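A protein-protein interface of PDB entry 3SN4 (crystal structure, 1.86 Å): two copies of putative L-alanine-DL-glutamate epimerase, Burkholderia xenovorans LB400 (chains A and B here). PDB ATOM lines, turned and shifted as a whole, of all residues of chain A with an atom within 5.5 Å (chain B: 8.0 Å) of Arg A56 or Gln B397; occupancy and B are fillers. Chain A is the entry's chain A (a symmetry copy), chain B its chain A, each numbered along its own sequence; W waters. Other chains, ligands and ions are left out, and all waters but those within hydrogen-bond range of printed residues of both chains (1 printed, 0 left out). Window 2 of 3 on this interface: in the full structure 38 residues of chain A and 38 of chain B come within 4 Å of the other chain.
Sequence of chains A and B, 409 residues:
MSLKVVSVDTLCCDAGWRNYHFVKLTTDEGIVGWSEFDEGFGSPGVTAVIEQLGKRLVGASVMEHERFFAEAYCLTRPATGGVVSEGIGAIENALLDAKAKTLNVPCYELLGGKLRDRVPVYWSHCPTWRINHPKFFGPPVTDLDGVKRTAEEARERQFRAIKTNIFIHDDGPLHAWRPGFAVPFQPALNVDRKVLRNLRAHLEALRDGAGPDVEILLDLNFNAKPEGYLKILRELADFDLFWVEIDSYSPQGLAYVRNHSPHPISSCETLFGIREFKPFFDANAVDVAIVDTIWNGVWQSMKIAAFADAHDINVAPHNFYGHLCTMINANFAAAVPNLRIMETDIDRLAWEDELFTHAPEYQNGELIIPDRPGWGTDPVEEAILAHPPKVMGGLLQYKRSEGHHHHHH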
ATOM      1  N   GLN A  52      29.281 -15.040  -1.009  1.00  0.00           N
ATOM      2  CA  GLN A  52      28.803 -15.405  -2.356  1.00  0.00           C
ATOM      3  C   GLN A  52      27.678 -16.424  -2.327  1.00  0.00           C
ATOM      4  O   GLN A  52      26.670 -16.263  -3.015  1.00  0.00           O
ATOM      5  CB  GLN A  52      29.914 -16.017  -3.224  1.00  0.00           C
ATOM      6  CG  GLN A  52      30.882 -15.065  -3.792  1.00  0.00           C
ATOM      7  CD  GLN A  52      30.245 -14.012  -4.641  1.00  0.00           C
ATOM      8  OE1 GLN A  52      29.313 -14.285  -5.416  1.00  0.00           O
ATOM      9  NE2 GLN A  52      30.732 -12.785  -4.492  1.00  0.00           N
ATOM     10  N   LEU A  53      27.885 -17.521  -1.593  1.00  0.00           N
ATOM     11  CA  LEU A  53      26.917 -18.596  -1.582  1.00  0.00           C
ATOM     12  C   LEU A  53      25.598 -18.178  -0.924  1.00  0.00           C
ATOM     13  O   LEU A  53      24.516 -18.616  -1.354  1.00  0.00           O
ATOM     14  CB  LEU A  53      27.509 -19.858  -0.930  1.00  0.00           C
ATOM     15  CG  LEU A  53      28.565 -20.563  -1.777  1.00  0.00           C
ATOM     16  CD1 LEU A  53      29.074 -21.831  -1.067  1.00  0.00           C
ATOM     17  CD2 LEU A  53      28.010 -20.927  -3.163  1.00  0.00           C
ATOM     18  N   GLY A  54      25.678 -17.336   0.105  1.00  0.00           N
ATOM     19  CA  GLY A  54      24.482 -16.827   0.774  1.00  0.00           C
ATOM     20  C   GLY A  54      23.571 -16.005  -0.125  1.00  0.00           C
ATOM     21  O   GLY A  54      22.351 -16.057   0.010  1.00  0.00           O
ATOM     22  N   LYS A  55      24.155 -15.261  -1.056  1.00  0.00           N
ATOM     23  CA  LYS A  55      23.370 -14.538  -2.039  1.00  0.00           C
ATOM     24  C   LYS A  55      22.406 -15.456  -2.800  1.00  0.00           C
ATOM     25  O   LYS A  55      21.290 -15.055  -3.102  1.00  0.00           O
ATOM     26  CB  LYS A  55      24.285 -13.799  -3.025  1.00  0.00           C
ATOM     27  CG  LYS A  55      24.999 -12.622  -2.403  1.00  0.00           C
ATOM     28  CD  LYS A  55      26.012 -11.984  -3.355  1.00  0.00           C
ATOM     29  CE  LYS A  55      26.672 -10.742  -2.721  1.00  0.00           C
ATOM     30  NZ  LYS A  55      25.711  -9.562  -2.603  1.00  0.00           N
ATOM     31  N   ARG A  56      22.836 -16.682  -3.089  1.00  0.00           N
ATOM     32  CA  ARG A  56      22.047 -17.611  -3.904  1.00  0.00           C
ATOM     33  C   ARG A  56      20.924 -18.197  -3.058  1.00  0.00           C
ATOM     34  O   ARG A  56      19.878 -18.589  -3.575  1.00  0.00           O
ATOM     35  CB  ARG A  56      22.924 -18.756  -4.435  1.00  0.00           C
ATOM     36  CG  ARG A  56      24.129 -18.353  -5.303  1.00  0.00           C
ATOM     37  CD  ARG A  56      23.681 -17.928  -6.701  1.00  0.00           C
ATOM     38  NE  ARG A  56      22.918 -18.978  -7.406  1.00  0.00           N
ATOM     39  CZ  ARG A  56      23.233 -19.498  -8.598  1.00  0.00           C
ATOM     40  NH1 ARG A  56      24.316 -19.092  -9.267  1.00  0.00           N
ATOM     41  NH2 ARG A  56      22.452 -20.439  -9.131  1.00  0.00           N
ATOM     42  N   LEU A  57      21.147 -18.239  -1.745  1.00  0.00           N
ATOM     43  CA  LEU A  57      20.212 -18.859  -0.820  1.00  0.00           C
ATOM     44  C   LEU A  57      18.992 -17.987  -0.496  1.00  0.00           C
ATOM     45  O   LEU A  57      17.867 -18.508  -0.330  1.00  0.00           O
ATOM     46  CB  LEU A  57      20.968 -19.271   0.443  1.00  0.00           C
ATOM     47  CG  LEU A  57      20.208 -20.040   1.528  1.00  0.00           C
ATOM     48  CD1 LEU A  57      19.570 -21.316   0.953  1.00  0.00           C
ATOM     49  CD2 LEU A  57      21.147 -20.346   2.695  1.00  0.00           C
ATOM     50  N   VAL A  58      19.169 -16.667  -0.431  1.00  0.00           N
ATOM     51  CA  VAL A  58      18.046 -15.778  -0.158  1.00  0.00           C
ATOM     52  C   VAL A  58      16.939 -16.025  -1.183  1.00  0.00           C
ATOM     53  O   VAL A  58      17.196 -16.066  -2.390  1.00  0.00           O
ATOM     54  CB  VAL A  58      18.476 -14.285  -0.207  1.00  0.00           C
ATOM     55  CG1 VAL A  58      17.280 -13.381  -0.029  1.00  0.00           C
ATOM     56  CG2 VAL A  58      19.585 -14.010   0.854  1.00  0.00           C
ATOM     57  N   ALA A  60      15.140 -18.831  -1.200  1.00  0.00           N
ATOM     58  CA  ALA A  60      14.916 -20.277  -1.158  1.00  0.00           C
ATOM     59  C   ALA A  60      14.298 -20.698   0.176  1.00  0.00           C
ATOM     60  O   ALA A  60      14.309 -19.948   1.146  1.00  0.00           O
ATOM     61  CB  ALA A  60      16.213 -21.007  -1.389  1.00  0.00           C
ATOM     62  N   ARG A  67      18.926 -29.494  -0.711  1.00  0.00           N
ATOM     63  CA  ARG A  67      18.843 -28.802  -1.999  1.00  0.00           C
ATOM     64  C   ARG A  67      19.936 -27.736  -2.110  1.00  0.00           C
ATOM     65  O   ARG A  67      20.617 -27.633  -3.121  1.00  0.00           O
ATOM     66  CB  ARG A  67      17.473 -28.140  -2.166  1.00  0.00           C
ATOM     67  CG  ARG A  67      17.247 -27.493  -3.524  1.00  0.00           C
ATOM     68  CD  ARG A  67      16.356 -26.254  -3.420  1.00  0.00           C
ATOM     69  NE  ARG A  67      16.940 -25.196  -2.590  1.00  0.00           N
ATOM     70  CZ  ARG A  67      17.900 -24.378  -2.999  1.00  0.00           C
ATOM     71  NH1 ARG A  67      18.388 -24.485  -4.224  1.00  0.00           N
ATOM     72  NH2 ARG A  67      18.379 -23.467  -2.184  1.00  0.00           N
ATOM     73  N   GLU A  71      23.066 -27.782  -4.786  1.00  0.00           N
ATOM     74  CA  GLU A  71      23.320 -26.663  -5.652  1.00  0.00           C
ATOM     75  C   GLU A  71      24.716 -26.068  -5.431  1.00  0.00           C
ATOM     76  O   GLU A  71      25.447 -25.812  -6.384  1.00  0.00           O
ATOM     77  CB  GLU A  71      22.290 -25.574  -5.440  1.00  0.00           C
ATOM     78  CG  GLU A  71      22.432 -24.477  -6.483  1.00  0.00           C
ATOM     79  CD  GLU A  71      21.180 -23.694  -6.634  1.00  0.00           C
ATOM     80  OE1 GLU A  71      20.744 -23.094  -5.615  1.00  0.00           O
ATOM     81  OE2 GLU A  71      20.632 -23.695  -7.767  1.00  0.00           O
ATOM     82  N   LEU A  75      27.912 -25.529  -7.948  1.00  0.00           N
ATOM     83  CA  LEU A  75      28.404 -24.196  -8.320  1.00  0.00           C
ATOM     84  C   LEU A  75      29.900 -24.064  -8.036  1.00  0.00           C
ATOM     85  O   LEU A  75      30.582 -23.254  -8.699  1.00  0.00           O
ATOM     86  CB  LEU A  75      27.638 -23.089  -7.587  1.00  0.00           C
ATOM     87  CG  LEU A  75      26.154 -22.935  -7.900  1.00  0.00           C
ATOM     88  CD1 LEU A  75      25.548 -21.863  -6.997  1.00  0.00           C
ATOM     89  CD2 LEU A  75      25.912 -22.621  -9.389  1.00  0.00           C
ATOM     90  N   ALA B  15      35.846  -9.017 -17.522  1.00  0.00           N
ATOM     91  CA  ALA B  15      36.019  -9.896 -18.677  1.00  0.00           C
ATOM     92  C   ALA B  15      34.649 -10.397 -19.192  1.00  0.00           C
ATOM     93  O   ALA B  15      34.520 -11.517 -19.673  1.00  0.00           O
ATOM     94  CB  ALA B  15      36.935 -11.065 -18.332  1.00  0.00           C
ATOM     95  N   GLY B  16      33.642  -9.544 -19.075  1.00  0.00           N
ATOM     96  CA  GLY B  16      32.336  -9.740 -19.697  1.00  0.00           C
ATOM     97  C   GLY B  16      31.352 -10.458 -18.792  1.00  0.00           C
ATOM     98  O   GLY B  16      30.520  -9.835 -18.121  1.00  0.00           O
ATOM     99  N   TRP B  17      31.454 -11.777 -18.823  1.00  0.00           N
ATOM    100  CA  TRP B  17      30.594 -12.688 -18.069  1.00  0.00           C
ATOM    101  C   TRP B  17      31.348 -13.230 -16.851  1.00  0.00           C
ATOM    102  O   TRP B  17      30.842 -14.092 -16.119  1.00  0.00           O
ATOM    103  CB  TRP B  17      30.129 -13.837 -18.986  1.00  0.00           C
ATOM    104  CG  TRP B  17      31.254 -14.613 -19.601  1.00  0.00           C
ATOM    105  CD1 TRP B  17      31.999 -14.262 -20.712  1.00  0.00           C
ATOM    106  CD2 TRP B  17      31.797 -15.856 -19.132  1.00  0.00           C
ATOM    107  NE1 TRP B  17      32.958 -15.222 -20.957  1.00  0.00           N
ATOM    108  CE2 TRP B  17      32.855 -16.208 -20.010  1.00  0.00           C
ATOM    109  CE3 TRP B  17      31.485 -16.714 -18.064  1.00  0.00           C
ATOM    110  CZ2 TRP B  17      33.610 -17.376 -19.844  1.00  0.00           C
ATOM    111  CZ3 TRP B  17      32.240 -17.898 -17.900  1.00  0.00           C
ATOM    112  CH2 TRP B  17      33.294 -18.210 -18.787  1.00  0.00           C
ATOM    113  N   ARG B  18      32.574 -12.732 -16.665  1.00  0.00           N
ATOM    114  CA  ARG B  18      33.421 -13.045 -15.524  1.00  0.00           C
ATOM    115  C   ARG B  18      34.465 -11.929 -15.389  1.00  0.00           C
ATOM    116  O   ARG B  18      34.593 -11.073 -16.274  1.00  0.00           O
ATOM    117  CB  ARG B  18      34.144 -14.367 -15.770  1.00  0.00           C
ATOM    118  CG  ARG B  18      35.087 -14.314 -16.984  1.00  0.00           C
ATOM    119  CD  ARG B  18      35.691 -15.671 -17.273  1.00  0.00           C
ATOM    120  NE  ARG B  18      36.390 -15.677 -18.561  1.00  0.00           N
ATOM    121  CZ  ARG B  18      37.194 -16.656 -18.985  1.00  0.00           C
ATOM    122  NH1 ARG B  18      37.437 -17.727 -18.217  1.00  0.00           N
ATOM    123  NH2 ARG B  18      37.780 -16.551 -20.186  1.00  0.00           N
ATOM    124  N   ASN B  19      35.228 -11.957 -14.303  1.00  0.00           N
ATOM    125  CA  ASN B  19      36.321 -11.000 -14.120  1.00  0.00           C
ATOM    126  C   ASN B  19      37.653 -11.677 -14.309  1.00  0.00           C
ATOM    127  O   ASN B  19      37.764 -12.899 -14.079  1.00  0.00           O
ATOM    128  CB  ASN B  19      36.290 -10.378 -12.729  1.00  0.00           C
ATOM    129  CG  ASN B  19      35.033  -9.589 -12.461  1.00  0.00           C
ATOM    130  OD1 ASN B  19      34.594  -8.770 -13.278  1.00  0.00           O
ATOM    131  ND2 ASN B  19      34.438  -9.826 -11.291  1.00  0.00           N
ATOM    132  N   GLY B  40      35.889 -17.087 -10.777  1.00  0.00           N
ATOM    133  CA  GLY B  40      34.591 -17.427 -11.327  1.00  0.00           C
ATOM    134  C   GLY B  40      34.404 -18.914 -11.534  1.00  0.00           C
ATOM    135  O   GLY B  40      33.273 -19.393 -11.505  1.00  0.00           O
ATOM    136  N   ASN B 132      27.257 -19.597 -25.805  1.00  0.00           N
ATOM    137  CA  ASN B 132      26.958 -19.278 -24.413  1.00  0.00           C
ATOM    138  C   ASN B 132      27.134 -17.808 -24.045  1.00  0.00           C
ATOM    139  O   ASN B 132      26.417 -17.294 -23.186  1.00  0.00           O
ATOM    140  CB  ASN B 132      27.820 -20.149 -23.504  1.00  0.00           C
ATOM    141  CG  ASN B 132      27.420 -21.609 -23.566  1.00  0.00           C
ATOM    142  OD1 ASN B 132      26.343 -21.939 -24.071  1.00  0.00           O
ATOM    143  ND2 ASN B 132      28.270 -22.485 -23.049  1.00  0.00           N
ATOM    144  N   HIS B 133      28.077 -17.128 -24.700  1.00  0.00           N
ATOM    145  CA  HIS B 133      28.366 -15.725 -24.387  1.00  0.00           C
ATOM    146  C   HIS B 133      28.408 -14.892 -25.674  1.00  0.00           C
ATOM    147  O   HIS B 133      29.413 -14.245 -25.977  1.00  0.00           O
ATOM    148  CB  HIS B 133      29.674 -15.650 -23.599  1.00  0.00           C
ATOM    149  CG  HIS B 133      29.712 -16.577 -22.425  1.00  0.00           C
ATOM    150  ND1 HIS B 133      28.914 -16.400 -21.312  1.00  0.00           N
ATOM    151  CD2 HIS B 133      30.425 -17.709 -22.203  1.00  0.00           C
ATOM    152  CE1 HIS B 133      29.148 -17.375 -20.449  1.00  0.00           C
ATOM    153  NE2 HIS B 133      30.062 -18.182 -20.963  1.00  0.00           N
ATOM    154  N   PHE B 136      29.599 -11.232 -26.073  1.00  0.00           N
ATOM    155  CA  PHE B 136      31.031 -10.948 -25.966  1.00  0.00           C
ATOM    156  C   PHE B 136      31.849 -11.538 -27.108  1.00  0.00           C
ATOM    157  O   PHE B 136      32.861 -10.944 -27.501  1.00  0.00           O
ATOM    158  CB  PHE B 136      31.547 -11.394 -24.601  1.00  0.00           C
ATOM    159  CG  PHE B 136      30.822 -10.743 -23.465  1.00  0.00           C
ATOM    160  CD1 PHE B 136      30.951  -9.382 -23.237  1.00  0.00           C
ATOM    161  CD2 PHE B 136      29.968 -11.474 -22.658  1.00  0.00           C
ATOM    162  CE1 PHE B 136      30.261  -8.763 -22.207  1.00  0.00           C
ATOM    163  CE2 PHE B 136      29.269 -10.865 -21.628  1.00  0.00           C
ATOM    164  CZ  PHE B 136      29.418  -9.509 -21.397  1.00  0.00           C
ATOM    165  N   PHE B 181      27.310 -28.112 -13.186  1.00  0.00           N
ATOM    166  CA  PHE B 181      27.439 -26.770 -12.635  1.00  0.00           C
ATOM    167  C   PHE B 181      26.058 -26.128 -12.358  1.00  0.00           C
ATOM    168  O   PHE B 181      25.906 -24.887 -12.274  1.00  0.00           O
ATOM    169  CB  PHE B 181      28.289 -25.912 -13.602  1.00  0.00           C
ATOM    170  CG  PHE B 181      29.691 -26.433 -13.864  1.00  0.00           C
ATOM    171  CD1 PHE B 181      30.438 -27.057 -12.862  1.00  0.00           C
ATOM    172  CD2 PHE B 181      30.310 -26.207 -15.109  1.00  0.00           C
ATOM    173  CE1 PHE B 181      31.747 -27.499 -13.091  1.00  0.00           C
ATOM    174  CE2 PHE B 181      31.618 -26.634 -15.353  1.00  0.00           C
ATOM    175  CZ  PHE B 181      32.346 -27.299 -14.336  1.00  0.00           C
ATOM    176  N   ALA B 182      25.049 -26.980 -12.170  1.00  0.00           N
ATOM    177  CA  ALA B 182      23.697 -26.536 -11.856  1.00  0.00           C
ATOM    178  C   ALA B 182      23.009 -25.686 -12.962  1.00  0.00           C
ATOM    179  O   ALA B 182      22.052 -24.962 -12.679  1.00  0.00           O
ATOM    180  CB  ALA B 182      23.661 -25.803 -10.469  1.00  0.00           C
ATOM    181  N   VAL B 183      23.473 -25.783 -14.210  1.00  0.00           N
ATOM    182  CA  VAL B 183      22.728 -25.224 -15.337  1.00  0.00           C
ATOM    183  C   VAL B 183      22.356 -26.296 -16.392  1.00  0.00           C
ATOM    184  O   VAL B 183      23.120 -26.556 -17.322  1.00  0.00           O
ATOM    185  CB  VAL B 183      23.485 -24.061 -16.008  1.00  0.00           C
ATOM    186  CG1 VAL B 183      22.603 -23.426 -17.090  1.00  0.00           C
ATOM    187  CG2 VAL B 183      23.870 -23.017 -14.960  1.00  0.00           C
ATOM    188  N   PHE B 185      19.652 -27.240 -12.911  1.00  0.00           N
ATOM    189  CA  PHE B 185      19.742 -27.960 -11.652  1.00  0.00           C
ATOM    190  C   PHE B 185      19.030 -29.293 -11.809  1.00  0.00           C
ATOM    191  O   PHE B 185      17.787 -29.395 -11.723  1.00  0.00           O
ATOM    192  CB  PHE B 185      19.154 -27.144 -10.492  1.00  0.00           C
ATOM    193  CG  PHE B 185      19.294 -27.820  -9.149  1.00  0.00           C
ATOM    194  CD1 PHE B 185      20.544 -27.937  -8.548  1.00  0.00           C
ATOM    195  CD2 PHE B 185      18.186 -28.355  -8.500  1.00  0.00           C
ATOM    196  CE1 PHE B 185      20.681 -28.572  -7.321  1.00  0.00           C
ATOM    197  CE2 PHE B 185      18.327 -28.998  -7.261  1.00  0.00           C
ATOM    198  CZ  PHE B 185      19.568 -29.092  -6.680  1.00  0.00           C
ATOM    199  N   LYS B 390      32.740  -6.548 -12.424  1.00  0.00           N
ATOM    200  CA  LYS B 390      31.339  -6.700 -11.997  1.00  0.00           C
ATOM    201  C   LYS B 390      31.365  -7.586 -10.780  1.00  0.00           C
ATOM    202  O   LYS B 390      32.439  -7.979 -10.328  1.00  0.00           O
ATOM    203  CB  LYS B 390      30.493  -7.333 -13.102  1.00  0.00           C
ATOM    204  CG  LYS B 390      30.318  -6.443 -14.324  1.00  0.00           C
ATOM    205  CD  LYS B 390      29.847  -7.267 -15.537  1.00  0.00           C
ATOM    206  CE  LYS B 390      29.764  -6.413 -16.805  1.00  0.00           C
ATOM    207  NZ  LYS B 390      29.736  -7.295 -18.004  1.00  0.00           N
ATOM    208  N   VAL B 391      30.195  -7.904 -10.236  1.00  0.00           N
ATOM    209  CA  VAL B 391      30.144  -8.875  -9.146  1.00  0.00           C
ATOM    210  C   VAL B 391      30.608 -10.208  -9.717  1.00  0.00           C
ATOM    211  O   VAL B 391      30.578 -10.389 -10.931  1.00  0.00           O
ATOM    212  CB  VAL B 391      28.732  -9.012  -8.576  1.00  0.00           C
ATOM    213  CG1 VAL B 391      28.296  -7.679  -7.901  1.00  0.00           C
ATOM    214  CG2 VAL B 391      27.775  -9.460  -9.683  1.00  0.00           C
ATOM    215  N   MET B 392      31.027 -11.147  -8.872  1.00  0.00           N
ATOM    216  CA  MET B 392      31.480 -12.442  -9.400  1.00  0.00           C
ATOM    217  C   MET B 392      30.519 -13.023 -10.448  1.00  0.00           C
ATOM    218  O   MET B 392      29.303 -13.028 -10.262  1.00  0.00           O
ATOM    219  CB  MET B 392      31.668 -13.461  -8.284  1.00  0.00           C
ATOM    220  CG  MET B 392      32.703 -14.518  -8.605  1.00  0.00           C
ATOM    221  SD  MET B 392      32.917 -15.655  -7.030  1.00  0.00           S
ATOM    222  CE  MET B 392      33.699 -14.359  -5.743  1.00  0.00           C
ATOM    223  N   GLY B 393      31.099 -13.531 -11.535  1.00  0.00           N
ATOM    224  CA  GLY B 393      30.364 -14.237 -12.574  1.00  0.00           C
ATOM    225  C   GLY B 393      30.826 -15.689 -12.651  1.00  0.00           C
ATOM    226  O   GLY B 393      30.882 -16.400 -11.625  1.00  0.00           O
ATOM    227  N   GLY B 394      31.150 -16.135 -13.865  1.00  0.00           N
ATOM    228  CA  GLY B 394      31.524 -17.536 -14.099  1.00  0.00           C
ATOM    229  C   GLY B 394      30.412 -18.494 -13.685  1.00  0.00           C
ATOM    230  O   GLY B 394      29.227 -18.265 -13.980  1.00  0.00           O
ATOM    231  N   LEU B 395      30.790 -19.552 -12.958  1.00  0.00           N
ATOM    232  CA  LEU B 395      29.818 -20.533 -12.424  1.00  0.00           C
ATOM    233  C   LEU B 395      28.854 -19.905 -11.438  1.00  0.00           C
ATOM    234  O   LEU B 395      27.732 -20.393 -11.267  1.00  0.00           O
ATOM    235  CB  LEU B 395      30.533 -21.702 -11.717  1.00  0.00           C
ATOM    236  CG  LEU B 395      31.567 -22.443 -12.537  1.00  0.00           C
ATOM    237  CD1 LEU B 395      31.994 -23.706 -11.783  1.00  0.00           C
ATOM    238  CD2 LEU B 395      31.057 -22.739 -13.983  1.00  0.00           C
ATOM    239  N   LEU B 396      29.298 -18.822 -10.798  1.00  0.00           N
ATOM    240  CA  LEU B 396      28.507 -18.132  -9.802  1.00  0.00           C
ATOM    241  C   LEU B 396      27.591 -17.040 -10.406  1.00  0.00           C
ATOM    242  O   LEU B 396      26.965 -16.301  -9.656  1.00  0.00           O
ATOM    243  CB  LEU B 396      29.428 -17.548  -8.714  1.00  0.00           C
ATOM    244  CG  LEU B 396      30.062 -18.500  -7.667  1.00  0.00           C
ATOM    245  CD1 LEU B 396      28.997 -19.213  -6.813  1.00  0.00           C
ATOM    246  CD2 LEU B 396      31.044 -19.507  -8.281  1.00  0.00           C
ATOM    247  N   GLN B 397      27.510 -16.952 -11.741  1.00  0.00           N
ATOM    248  CA  GLN B 397      26.572 -16.047 -12.435  1.00  0.00           C
ATOM    249  C   GLN B 397      25.209 -16.700 -12.548  1.00  0.00           C
ATOM    250  O   GLN B 397      24.706 -17.252 -11.571  1.00  0.00           O
ATOM    251  CB  GLN B 397      27.077 -15.710 -13.847  1.00  0.00           C
ATOM    252  CG  GLN B 397      26.316 -14.574 -14.536  1.00  0.00           C
ATOM    253  CD  GLN B 397      27.176 -13.817 -15.556  1.00  0.00           C
ATOM    254  OE1 GLN B 397      27.099 -12.583 -15.678  1.00  0.00           O
ATOM    255  NE2 GLN B 397      28.004 -14.558 -16.286  1.00  0.00           N
HETATM  256  O   HOH W   1      30.744 -10.534  -6.091  1.00  0.00           O
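O of Trp B17 lies within hydrogen-bond range of NE2 of Gln B397, at 2.9 Å.
The backbone carbonyl oxygen (O) of Gly B40 is in hydrogen-bond range of the backbone NH (N) of Leu B395 (2.9 Å).
NH1 of Arg A67 is in salt-bridge range of OE1 of Glu A71 (3.1 Å).
The side-chain carboxylate of Glu A71 is in salt-bridge range of the guanidinium group of Arg A56, 3.97 Å away.
O of Gln B397 lies within hydrogen-bond range of NH1 of Arg A56 (3.0 Å).
Printed residues of chain B within 4 Å of Arg A56: Leu B396 and Gln B397.
Of the printed residues of chain B, Leu A75 touches Phe B181, Leu B395 and Leu B396.
Of the printed residues of chain A, Leu B396 touches Arg A56 and Leu A75.
Gln B397 touches just one residue of chain A: Arg A56 (3.0 Å).
The nearest residue of chain B that does not touch Arg A56 is Leu B395 (4.2 Å).
The nearest printed residue of chain A that does not touch Gln B397 is Leu A75 (5.9 Å).
The nearest printed residue of chain A that does not touch Phe B181 is Glu A71 (6.0 Å).
Of the 21 printed residues of chain B, 6 touch a printed residue of chain A.
Printed residues of chain B that touch a printed residue of chain A: Phe B181, Phe B185, Met B392, Leu B395, Leu B396 and Gln B397.
Of the 11 printed residues of chain A, 5 touch a printed residue of chain B.
Hydrophobic or aromatic side chains of chain A that line the printed part of chain B: Leu A75.
Among the printed residues, no Asp or Glu carboxylate lies within 4 Å of a Lys or Arg side-chain nitrogen of the other chain.
No position is printed for both chains.
Water W1 bridges the side-chain amide nitrogen (NE2) of Gln A52 (2.8 Å) and the backbone NH (N) of Met B392 (2.9 Å).
Gln A52 touches Met B392.
Leu B396 touches Arg A56.
O of Arg A67 touches CZ of Phe B185, at 3.99 Å.
Phe B185 touches Glu A71.
Phe B181 touches Leu A75 (O to CD2, 3.7 Å).
Leu A75 touches Leu B395 (O to CB, 3.4 Å).
Leu B396 touches Leu A75 (CD2 to O, 3.8 Å).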
